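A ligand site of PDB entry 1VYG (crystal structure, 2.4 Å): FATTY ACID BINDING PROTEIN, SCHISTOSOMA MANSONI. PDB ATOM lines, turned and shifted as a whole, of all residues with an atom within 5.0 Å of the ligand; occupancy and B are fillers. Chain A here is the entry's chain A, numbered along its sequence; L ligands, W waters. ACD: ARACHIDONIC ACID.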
ATOM      1  N   PHE A  18     -10.716  36.946  17.687  1.00  0.00           N
ATOM      2  CA  PHE A  18     -10.082  35.636  17.515  1.00  0.00           C
ATOM      3  C   PHE A  18      -8.567  35.672  17.679  1.00  0.00           C
ATOM      4  O   PHE A  18      -7.957  34.678  18.080  1.00  0.00           O
ATOM      5  CB  PHE A  18     -10.449  35.027  16.155  1.00  0.00           C
ATOM      6  CG  PHE A  18     -10.065  33.570  15.997  1.00  0.00           C
ATOM      7  CD1 PHE A  18      -9.367  33.151  14.882  1.00  0.00           C
ATOM      8  CD2 PHE A  18     -10.426  32.624  16.938  1.00  0.00           C
ATOM      9  CE1 PHE A  18      -9.016  31.818  14.719  1.00  0.00           C
ATOM     10  CE2 PHE A  18     -10.073  31.284  16.782  1.00  0.00           C
ATOM     11  CZ  PHE A  18      -9.377  30.879  15.680  1.00  0.00           C
ATOM     12  N   VAL A  21      -7.616  34.978  21.365  1.00  0.00           N
ATOM     13  CA  VAL A  21      -7.693  33.655  21.969  1.00  0.00           C
ATOM     14  C   VAL A  21      -6.491  32.848  21.577  1.00  0.00           C
ATOM     15  O   VAL A  21      -5.989  32.052  22.378  1.00  0.00           O
ATOM     16  CB  VAL A  21      -8.974  32.813  21.664  1.00  0.00           C
ATOM     17  CG1 VAL A  21     -10.234  33.625  21.818  1.00  0.00           C
ATOM     18  CG2 VAL A  21      -8.891  32.102  20.271  1.00  0.00           C
ATOM     19  N   MET A  22      -6.016  33.054  20.371  1.00  0.00           N
ATOM     20  CA  MET A  22      -4.993  32.186  19.857  1.00  0.00           C
ATOM     21  C   MET A  22      -3.571  32.805  19.840  1.00  0.00           C
ATOM     22  O   MET A  22      -2.619  32.139  19.525  1.00  0.00           O
ATOM     23  CB  MET A  22      -5.384  31.665  18.487  1.00  0.00           C
ATOM     24  CG  MET A  22      -5.352  32.688  17.425  1.00  0.00           C
ATOM     25  SD  MET A  22      -6.065  31.990  15.968  1.00  0.00           S
ATOM     26  CE  MET A  22      -5.916  33.452  14.835  1.00  0.00           C
ATOM     27  N   LEU A  25      -3.077  31.142  22.955  1.00  0.00           N
ATOM     28  CA  LEU A  25      -2.715  29.743  22.703  1.00  0.00           C
ATOM     29  C   LEU A  25      -1.271  29.568  22.237  1.00  0.00           C
ATOM     30  O   LEU A  25      -0.814  28.452  22.043  1.00  0.00           O
ATOM     31  CB  LEU A  25      -3.666  29.115  21.681  1.00  0.00           C
ATOM     32  CG  LEU A  25      -5.085  28.985  22.254  1.00  0.00           C
ATOM     33  CD1 LEU A  25      -6.096  28.763  21.157  1.00  0.00           C
ATOM     34  CD2 LEU A  25      -5.138  27.847  23.315  1.00  0.00           C
ATOM     35  N   VAL A  27      -0.250  30.186  19.370  1.00  0.00           N
ATOM     36  CA  VAL A  27      -0.209  29.975  17.925  1.00  0.00           C
ATOM     37  C   VAL A  27       0.843  30.915  17.373  1.00  0.00           C
ATOM     38  O   VAL A  27       0.920  32.072  17.812  1.00  0.00           O
ATOM     39  CB  VAL A  27      -1.558  30.243  17.254  1.00  0.00           C
ATOM     40  CG1 VAL A  27      -1.473  30.040  15.735  1.00  0.00           C
ATOM     41  CG2 VAL A  27      -2.614  29.324  17.826  1.00  0.00           C
ATOM     42  N   THR A  31       0.738  31.423  11.694  1.00  0.00           N
ATOM     43  CA  THR A  31      -0.471  30.616  11.659  1.00  0.00           C
ATOM     44  C   THR A  31      -1.634  31.460  12.153  1.00  0.00           C
ATOM     45  O   THR A  31      -2.733  31.332  11.645  1.00  0.00           O
ATOM     46  CB  THR A  31      -0.295  29.324  12.446  1.00  0.00           C
ATOM     47  OG1 THR A  31       0.739  28.543  11.828  1.00  0.00           O
ATOM     48  CG2 THR A  31      -1.503  28.412  12.332  1.00  0.00           C
ATOM     49  N   ILE A  34      -2.934  33.589   9.200  1.00  0.00           N
ATOM     50  CA  ILE A  34      -3.800  32.700   8.413  1.00  0.00           C
ATOM     51  C   ILE A  34      -5.130  32.460   9.121  1.00  0.00           C
ATOM     52  O   ILE A  34      -6.159  32.426   8.484  1.00  0.00           O
ATOM     53  CB  ILE A  34      -3.138  31.336   8.143  1.00  0.00           C
ATOM     54  CG1 ILE A  34      -1.811  31.492   7.375  1.00  0.00           C
ATOM     55  CG2 ILE A  34      -4.069  30.413   7.333  1.00  0.00           C
ATOM     56  CD1 ILE A  34      -1.977  31.870   5.939  1.00  0.00           C
ATOM     57  N   GLY A  35      -5.109  32.288  10.441  1.00  0.00           N
ATOM     58  CA  GLY A  35      -6.334  32.145  11.217  1.00  0.00           C
ATOM     59  C   GLY A  35      -7.276  33.324  11.079  1.00  0.00           C
ATOM     60  O   GLY A  35      -8.486  33.175  11.011  1.00  0.00           O
ATOM     61  N   VAL A  38      -8.500  33.268   6.717  1.00  0.00           N
ATOM     62  CA  VAL A  38      -9.296  32.226   6.062  1.00  0.00           C
ATOM     63  C   VAL A  38     -10.666  32.038   6.678  1.00  0.00           C
ATOM     64  O   VAL A  38     -10.889  32.287   7.868  1.00  0.00           O
ATOM     65  CB  VAL A  38      -8.604  30.850   6.032  1.00  0.00           C
ATOM     66  CG1 VAL A  38      -7.132  30.994   5.675  1.00  0.00           C
ATOM     67  CG2 VAL A  38      -8.780  30.128   7.362  1.00  0.00           C
ATOM     68  N   PRO A  40     -13.084  29.064   6.991  1.00  0.00           N
ATOM     69  CA  PRO A  40     -13.287  27.636   6.856  1.00  0.00           C
ATOM     70  C   PRO A  40     -14.728  27.294   6.590  1.00  0.00           C
ATOM     71  O   PRO A  40     -15.634  28.087   6.853  1.00  0.00           O
ATOM     72  CB  PRO A  40     -12.869  27.109   8.222  1.00  0.00           C
ATOM     73  CG  PRO A  40     -12.108  28.147   8.815  1.00  0.00           C
ATOM     74  CD  PRO A  40     -12.728  29.408   8.379  1.00  0.00           C
ATOM     75  N   VAL A  42     -17.025  24.192   7.740  1.00  0.00           N
ATOM     76  CA  VAL A  42     -17.150  22.980   8.525  1.00  0.00           C
ATOM     77  C   VAL A  42     -18.441  22.242   8.165  1.00  0.00           C
ATOM     78  O   VAL A  42     -19.465  22.831   7.885  1.00  0.00           O
ATOM     79  CB  VAL A  42     -16.974  23.215  10.049  1.00  0.00           C
ATOM     80  CG1 VAL A  42     -16.158  24.475  10.316  1.00  0.00           C
ATOM     81  CG2 VAL A  42     -18.269  23.286  10.775  1.00  0.00           C
ATOM     82  N   MET A  53     -16.955  16.073  12.374  1.00  0.00           N
ATOM     83  CA  MET A  53     -16.861  17.476  12.027  1.00  0.00           C
ATOM     84  C   MET A  53     -15.643  17.657  11.122  1.00  0.00           C
ATOM     85  O   MET A  53     -14.512  17.491  11.566  1.00  0.00           O
ATOM     86  CB  MET A  53     -16.713  18.338  13.279  1.00  0.00           C
ATOM     87  CG  MET A  53     -16.631  19.827  12.943  1.00  0.00           C
ATOM     88  SD  MET A  53     -16.257  20.921  14.305  1.00  0.00           S
ATOM     89  CE  MET A  53     -14.905  21.790  13.627  1.00  0.00           C
ATOM     90  N   THR A  55     -13.392  20.234   8.797  1.00  0.00           N
ATOM     91  CA  THR A  55     -13.098  21.649   8.538  1.00  0.00           C
ATOM     92  C   THR A  55     -12.220  21.779   7.320  1.00  0.00           C
ATOM     93  O   THR A  55     -11.190  21.112   7.228  1.00  0.00           O
ATOM     94  CB  THR A  55     -12.408  22.296   9.764  1.00  0.00           C
ATOM     95  OG1 THR A  55     -13.304  22.290  10.891  1.00  0.00           O
ATOM     96  CG2 THR A  55     -12.110  23.816   9.528  1.00  0.00           C
ATOM     97  N   SER A  57     -10.265  24.552   4.901  1.00  0.00           N
ATOM     98  CA  SER A  57      -9.776  25.853   4.481  1.00  0.00           C
ATOM     99  C   SER A  57      -8.646  25.641   3.502  1.00  0.00           C
ATOM    100  O   SER A  57      -8.275  24.506   3.193  1.00  0.00           O
ATOM    101  CB  SER A  57      -9.298  26.669   5.690  1.00  0.00           C
ATOM    102  OG  SER A  57      -8.366  25.928   6.465  1.00  0.00           O
ATOM    103  N   PHE A  59      -5.740  26.521   4.391  1.00  0.00           N
ATOM    104  CA  PHE A  59      -4.659  26.146   5.281  1.00  0.00           C
ATOM    105  C   PHE A  59      -4.550  24.627   5.410  1.00  0.00           C
ATOM    106  O   PHE A  59      -3.605  24.018   4.901  1.00  0.00           O
ATOM    107  CB  PHE A  59      -4.859  26.788   6.649  1.00  0.00           C
ATOM    108  CG  PHE A  59      -3.774  26.498   7.626  1.00  0.00           C
ATOM    109  CD1 PHE A  59      -4.071  26.108   8.917  1.00  0.00           C
ATOM    110  CD2 PHE A  59      -2.435  26.635   7.263  1.00  0.00           C
ATOM    111  CE1 PHE A  59      -3.089  25.839   9.821  1.00  0.00           C
ATOM    112  CE2 PHE A  59      -1.439  26.392   8.171  1.00  0.00           C
ATOM    113  CZ  PHE A  59      -1.766  25.994   9.451  1.00  0.00           C
ATOM    114  N   LYS A  60      -5.529  24.034   6.097  1.00  0.00           N
ATOM    115  CA  LYS A  60      -5.645  22.588   6.249  1.00  0.00           C
ATOM    116  C   LYS A  60      -7.088  22.161   6.087  1.00  0.00           C
ATOM    117  O   LYS A  60      -8.023  22.939   6.317  1.00  0.00           O
ATOM    118  CB  LYS A  60      -5.174  22.179   7.634  1.00  0.00           C
ATOM    119  CG  LYS A  60      -3.754  22.568   7.934  1.00  0.00           C
ATOM    120  CD  LYS A  60      -3.268  22.051   9.261  1.00  0.00           C
ATOM    121  CE  LYS A  60      -1.772  22.308   9.393  1.00  0.00           C
ATOM    122  NZ  LYS A  60      -1.269  22.135  10.800  1.00  0.00           N
ATOM    123  N   LEU A  62      -8.769  19.469   8.125  1.00  0.00           N
ATOM    124  CA  LEU A  62      -8.780  18.443   9.164  1.00  0.00           C
ATOM    125  C   LEU A  62     -10.182  17.909   9.346  1.00  0.00           C
ATOM    126  O   LEU A  62     -11.163  18.550   8.990  1.00  0.00           O
ATOM    127  CB  LEU A  62      -8.306  18.993  10.507  1.00  0.00           C
ATOM    128  CG  LEU A  62      -7.045  19.870  10.507  1.00  0.00           C
ATOM    129  CD1 LEU A  62      -7.331  21.211  11.190  1.00  0.00           C
ATOM    130  CD2 LEU A  62      -5.839  19.161  11.159  1.00  0.00           C
ATOM    131  N   SER A  77      -5.513  22.508  14.159  1.00  0.00           N
ATOM    132  CA  SER A  77      -5.068  23.047  12.873  1.00  0.00           C
ATOM    133  C   SER A  77      -3.692  23.673  12.986  1.00  0.00           C
ATOM    134  O   SER A  77      -2.862  23.488  12.121  1.00  0.00           O
ATOM    135  CB  SER A  77      -6.059  24.074  12.342  1.00  0.00           C
ATOM    136  OG  SER A  77      -6.329  25.106  13.282  1.00  0.00           O
ATOM    137  N   ASP A  78      -3.371  24.323  13.985  1.00  0.00           N
ATOM    138  CA  ASP A  78      -2.205  25.044  14.409  1.00  0.00           C
ATOM    139  C   ASP A  78      -1.110  24.099  14.817  1.00  0.00           C
ATOM    140  O   ASP A  78       0.088  24.352  14.817  1.00  0.00           O
ATOM    141  CB  ASP A  78      -2.441  26.090  15.460  1.00  0.00           C
ATOM    142  CG  ASP A  78      -2.809  25.470  16.788  1.00  0.00           C
ATOM    143  OD1 ASP A  78      -1.917  25.284  17.600  1.00  0.00           O
ATOM    144  OD2 ASP A  78      -3.979  25.150  16.939  1.00  0.00           O
ATOM    145  N   ARG A  80      -1.246  21.801  17.779  1.00  0.00           N
ATOM    146  CA  ARG A  80      -1.083  21.303  19.165  1.00  0.00           C
ATOM    147  C   ARG A  80      -1.748  19.905  19.209  1.00  0.00           C
ATOM    148  O   ARG A  80      -2.715  19.586  18.548  1.00  0.00           O
ATOM    149  CB  ARG A  80      -1.743  22.275  20.100  1.00  0.00           C
ATOM    150  CG  ARG A  80      -1.139  23.644  20.103  1.00  0.00           C
ATOM    151  CD  ARG A  80      -2.146  24.652  20.943  1.00  0.00           C
ATOM    152  NE  ARG A  80      -3.318  25.016  20.207  1.00  0.00           N
ATOM    153  CZ  ARG A  80      -4.571  24.765  20.472  1.00  0.00           C
ATOM    154  NH1 ARG A  80      -5.502  25.138  19.646  1.00  0.00           N
ATOM    155  NH2 ARG A  80      -4.900  24.177  21.584  1.00  0.00           N
ATOM    156  N   GLN A  98     -10.685  21.396  24.807  1.00  0.00           N
ATOM    157  CA  GLN A  98      -9.458  20.981  24.166  1.00  0.00           C
ATOM    158  C   GLN A  98      -8.370  21.243  25.179  1.00  0.00           C
ATOM    159  O   GLN A  98      -8.099  22.390  25.537  1.00  0.00           O
ATOM    160  CB  GLN A  98      -9.183  21.813  22.903  1.00  0.00           C
ATOM    161  CG  GLN A  98      -9.799  21.237  21.661  1.00  0.00           C
ATOM    162  CD  GLN A  98      -9.507  22.052  20.419  1.00  0.00           C
ATOM    163  OE1 GLN A  98      -9.484  23.275  20.468  1.00  0.00           O
ATOM    164  NE2 GLN A  98      -9.282  21.382  19.307  1.00  0.00           N
ATOM    165  N   THR A 105      -8.846  25.057  25.809  1.00  0.00           N
ATOM    166  CA  THR A 105      -9.807  25.772  24.952  1.00  0.00           C
ATOM    167  C   THR A 105     -11.174  25.110  24.996  1.00  0.00           C
ATOM    168  O   THR A 105     -11.301  23.946  24.716  1.00  0.00           O
ATOM    169  CB  THR A 105      -9.316  25.812  23.483  1.00  0.00           C
ATOM    170  OG1 THR A 105      -7.983  26.317  23.406  1.00  0.00           O
ATOM    171  CG2 THR A 105     -10.135  26.815  22.646  1.00  0.00           C
ATOM    172  N   ILE A 107     -14.921  25.243  23.299  1.00  0.00           N
ATOM    173  CA  ILE A 107     -15.500  25.710  22.065  1.00  0.00           C
ATOM    174  C   ILE A 107     -16.964  25.328  22.072  1.00  0.00           C
ATOM    175  O   ILE A 107     -17.321  24.176  21.804  1.00  0.00           O
ATOM    176  CB  ILE A 107     -14.773  25.082  20.867  1.00  0.00           C
ATOM    177  CG1 ILE A 107     -13.308  25.493  20.844  1.00  0.00           C
ATOM    178  CG2 ILE A 107     -15.396  25.498  19.575  1.00  0.00           C
ATOM    179  CD1 ILE A 107     -12.392  24.370  20.505  1.00  0.00           C
ATOM    180  N   ARG A 109     -20.255  25.468  20.244  1.00  0.00           N
ATOM    181  CA  ARG A 109     -20.932  25.628  18.974  1.00  0.00           C
ATOM    182  C   ARG A 109     -22.421  25.483  19.226  1.00  0.00           C
ATOM    183  O   ARG A 109     -22.855  24.533  19.830  1.00  0.00           O
ATOM    184  CB  ARG A 109     -20.521  24.558  17.972  1.00  0.00           C
ATOM    185  CG  ARG A 109     -19.016  24.516  17.687  1.00  0.00           C
ATOM    186  CD  ARG A 109     -18.636  23.573  16.574  1.00  0.00           C
ATOM    187  NE  ARG A 109     -17.273  23.840  16.167  1.00  0.00           N
ATOM    188  CZ  ARG A 109     -16.195  23.427  16.846  1.00  0.00           C
ATOM    189  NH1 ARG A 109     -16.296  22.672  17.933  1.00  0.00           N
ATOM    190  NH2 ARG A 109     -14.996  23.759  16.423  1.00  0.00           N
ATOM    191  N   THR A 118     -19.967  29.918  17.169  1.00  0.00           N
ATOM    192  CA  THR A 118     -18.878  29.206  17.785  1.00  0.00           C
ATOM    193  C   THR A 118     -18.228  30.176  18.749  1.00  0.00           C
ATOM    194  O   THR A 118     -17.628  31.133  18.334  1.00  0.00           O
ATOM    195  CB  THR A 118     -17.858  28.765  16.745  1.00  0.00           C
ATOM    196  OG1 THR A 118     -18.428  27.733  15.936  1.00  0.00           O
ATOM    197  CG2 THR A 118     -16.645  28.109  17.401  1.00  0.00           C
ATOM    198  N   VAL A 120     -15.330  30.645  21.439  1.00  0.00           N
ATOM    199  CA  VAL A 120     -14.082  30.017  21.823  1.00  0.00           C
ATOM    200  C   VAL A 120     -13.453  30.734  23.021  1.00  0.00           C
ATOM    201  O   VAL A 120     -13.240  31.925  22.997  1.00  0.00           O
ATOM    202  CB  VAL A 120     -13.091  29.930  20.653  1.00  0.00           C
ATOM    203  CG1 VAL A 120     -11.954  29.008  21.001  1.00  0.00           C
ATOM    204  CG2 VAL A 120     -13.797  29.417  19.399  1.00  0.00           C
ATOM    205  N   ARG A 129     -17.348  33.197  16.723  1.00  0.00           N
ATOM    206  CA  ARG A 129     -17.260  32.970  15.304  1.00  0.00           C
ATOM    207  C   ARG A 129     -18.589  32.496  14.805  1.00  0.00           C
ATOM    208  O   ARG A 129     -19.094  31.499  15.253  1.00  0.00           O
ATOM    209  CB  ARG A 129     -16.145  31.968  15.026  1.00  0.00           C
ATOM    210  CG  ARG A 129     -14.815  32.685  14.946  1.00  0.00           C
ATOM    211  CD  ARG A 129     -13.639  31.855  15.322  1.00  0.00           C
ATOM    212  NE  ARG A 129     -13.232  30.942  14.255  1.00  0.00           N
ATOM    213  CZ  ARG A 129     -12.594  31.305  13.152  1.00  0.00           C
ATOM    214  NH1 ARG A 129     -12.273  30.370  12.268  1.00  0.00           N
ATOM    215  NH2 ARG A 129     -12.278  32.559  12.907  1.00  0.00           N
ATOM    216  N   TYR A 131     -20.955  31.121  11.714  1.00  0.00           N
ATOM    217  CA  TYR A 131     -20.988  30.415  10.469  1.00  0.00           C
ATOM    218  C   TYR A 131     -22.399  30.544   9.872  1.00  0.00           C
ATOM    219  O   TYR A 131     -23.375  30.332  10.553  1.00  0.00           O
ATOM    220  CB  TYR A 131     -20.607  28.951  10.701  1.00  0.00           C
ATOM    221  CG  TYR A 131     -19.127  28.718  10.995  1.00  0.00           C
ATOM    222  CD1 TYR A 131     -18.287  28.196  10.033  1.00  0.00           C
ATOM    223  CD2 TYR A 131     -18.575  29.029  12.240  1.00  0.00           C
ATOM    224  CE1 TYR A 131     -16.945  27.969  10.291  1.00  0.00           C
ATOM    225  CE2 TYR A 131     -17.235  28.809  12.504  1.00  0.00           C
ATOM    226  CZ  TYR A 131     -16.428  28.284  11.509  1.00  0.00           C
ATOM    227  OH  TYR A 131     -15.102  28.066  11.725  1.00  0.00           O
HETATM  228  C1  ACD L   1     -14.242  27.011  14.804  1.00  0.00           C
HETATM  229  C2  ACD L   1     -13.550  27.237  16.109  1.00  0.00           C
HETATM  230  C3  ACD L   1     -12.216  26.492  16.075  1.00  0.00           C
HETATM  231  C4  ACD L   1     -11.169  27.283  16.857  1.00  0.00           C
HETATM  232  C5  ACD L   1     -10.769  26.566  18.141  1.00  0.00           C
HETATM  233  C6  ACD L   1      -9.632  26.935  18.756  1.00  0.00           C
HETATM  234  C7  ACD L   1      -8.770  28.045  18.205  1.00  0.00           C
HETATM  235  C8  ACD L   1      -7.391  27.498  18.236  1.00  0.00           C
HETATM  236  C9  ACD L   1      -6.491  27.569  17.262  1.00  0.00           C
HETATM  237  C10 ACD L   1      -6.657  28.207  15.919  1.00  0.00           C
HETATM  238  C11 ACD L   1      -5.242  28.464  15.475  1.00  0.00           C
HETATM  239  C12 ACD L   1      -4.927  28.973  14.297  1.00  0.00           C
HETATM  240  C13 ACD L   1      -5.977  29.315  13.287  1.00  0.00           C
HETATM  241  C14 ACD L   1      -5.644  28.623  11.985  1.00  0.00           C
HETATM  242  C15 ACD L   1      -6.562  28.402  11.040  1.00  0.00           C
HETATM  243  C16 ACD L   1      -8.010  28.856  11.166  1.00  0.00           C
HETATM  244  C17 ACD L   1      -8.950  27.670  11.193  1.00  0.00           C
HETATM  245  C18 ACD L   1      -8.799  26.814   9.938  1.00  0.00           C
HETATM  246  C19 ACD L   1      -8.324  25.433  10.352  1.00  0.00           C
HETATM  247  C20 ACD L   1      -8.062  24.521   9.152  1.00  0.00           C
HETATM  248  O1  ACD L   1     -14.634  25.891  14.450  1.00  0.00           O
HETATM  249  O2  ACD L   1     -14.409  28.073  14.027  1.00  0.00           O
HETATM  250  O   HOH W   1     -13.772  24.381  12.581  1.00  0.00           O
HETATM  251  O   HOH W   2     -17.080  25.923  14.106  1.00  0.00           O
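Phe 18 touches the ligand (CE2 to C7, 3.8 Å).
Met 22 touches the ligand.
Leu 25 touches the ligand.
CG2 of Val 27 touches C11 of the ligand, 3.6 Å away.
Thr 31 touches the ligand.
CA of Gly 35 touches C13 of the ligand, at 3.5 Å.
Pro 40 touches the ligand.
Ser 57 touches the ligand.
Phe 59 touches the ligand.
O of Lys 60 touches C20 of the ligand, at 3.2 Å.
Leu 62 touches the ligand.
Ser 77 touches the ligand (CB to C19, 3.3 Å).
OD2 of Asp 78 touches C9 of the ligand (3.5 Å).
Arg 80 touches the ligand (NH1 to C8, 3.3 Å).
Thr 105 touches the ligand (CG2 to C6, 3.9 Å).
CD1 of Ile 107 touches C5 of the ligand (3.6 Å).
Thr 118 touches the ligand (CG2 to C2, 3.5 Å).
CG1 of Val 120 touches C6 of the ligand, at 3.8 Å.
Within 4 Å of the ligand: Phe 18, Met 22, Leu 25, Val 27, Thr 31, Gly 35, Pro 40, Ser 57, Phe 59, Lys 60, Leu 62, Ser 77, Asp 78, Arg 80, Thr 105, Ile 107, Arg 109, Thr 118, Val 120, Arg 129 and Tyr 131.
The nearest printed residue that does not touch the ligand is Gln 98 (4.04 Å).
Water W2 lies within hydrogen-bond range of an oxygen (O1) of the ligand, the side-chain hydroxyl of Thr 118 and the guanidinium group of Arg 109.
Water W1 lies within hydrogen-bond range of an oxygen (O1) of the ligand (2.6 Å) and the side-chain hydroxyl of Thr 55 (2.7 Å).
NZ of Lys 60 lies within hydrogen-bond range of O of Ser 77 (2.5 Å).
N of Thr 118 sits at hydrogen-bond distance from O of Arg 129 (2.6 Å).
The side-chain hydroxyl (OG) of Ser 57 lies close to the backbone NH (N) of Phe 59 (3.4 Å).
NE of Arg 109 lies close to SD of Met 53 (3.6 Å).
N of Gln 98 is in hydrogen-bond range of O of Thr 105, 2.6 Å away.
The backbone NH of Val 27 sits at hydrogen-bond distance from the backbone carbonyl oxygen of Met 22 (3.1 Å).
N of Thr 55 sits at hydrogen-bond distance from O of Leu 62 (2.8 Å).
The backbone carbonyl oxygen (O) of Lys 60 sits at hydrogen-bond distance from the side-chain hydroxyl (OG) of Ser 57, 3.0 Å away.
The guanidinium group (NE) of Arg 129 lies within salt-bridge range of an oxygen (O2) of the ligand, at 3.1 Å.
The side-chain hydroxyl (OH) of Tyr 131 sits at hydrogen-bond distance from an oxygen (O2) of the ligand, 2.4 Å away.
NH2 of Arg 109 lies within salt-bridge range of O1 of the ligand, 2.9 Å away.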
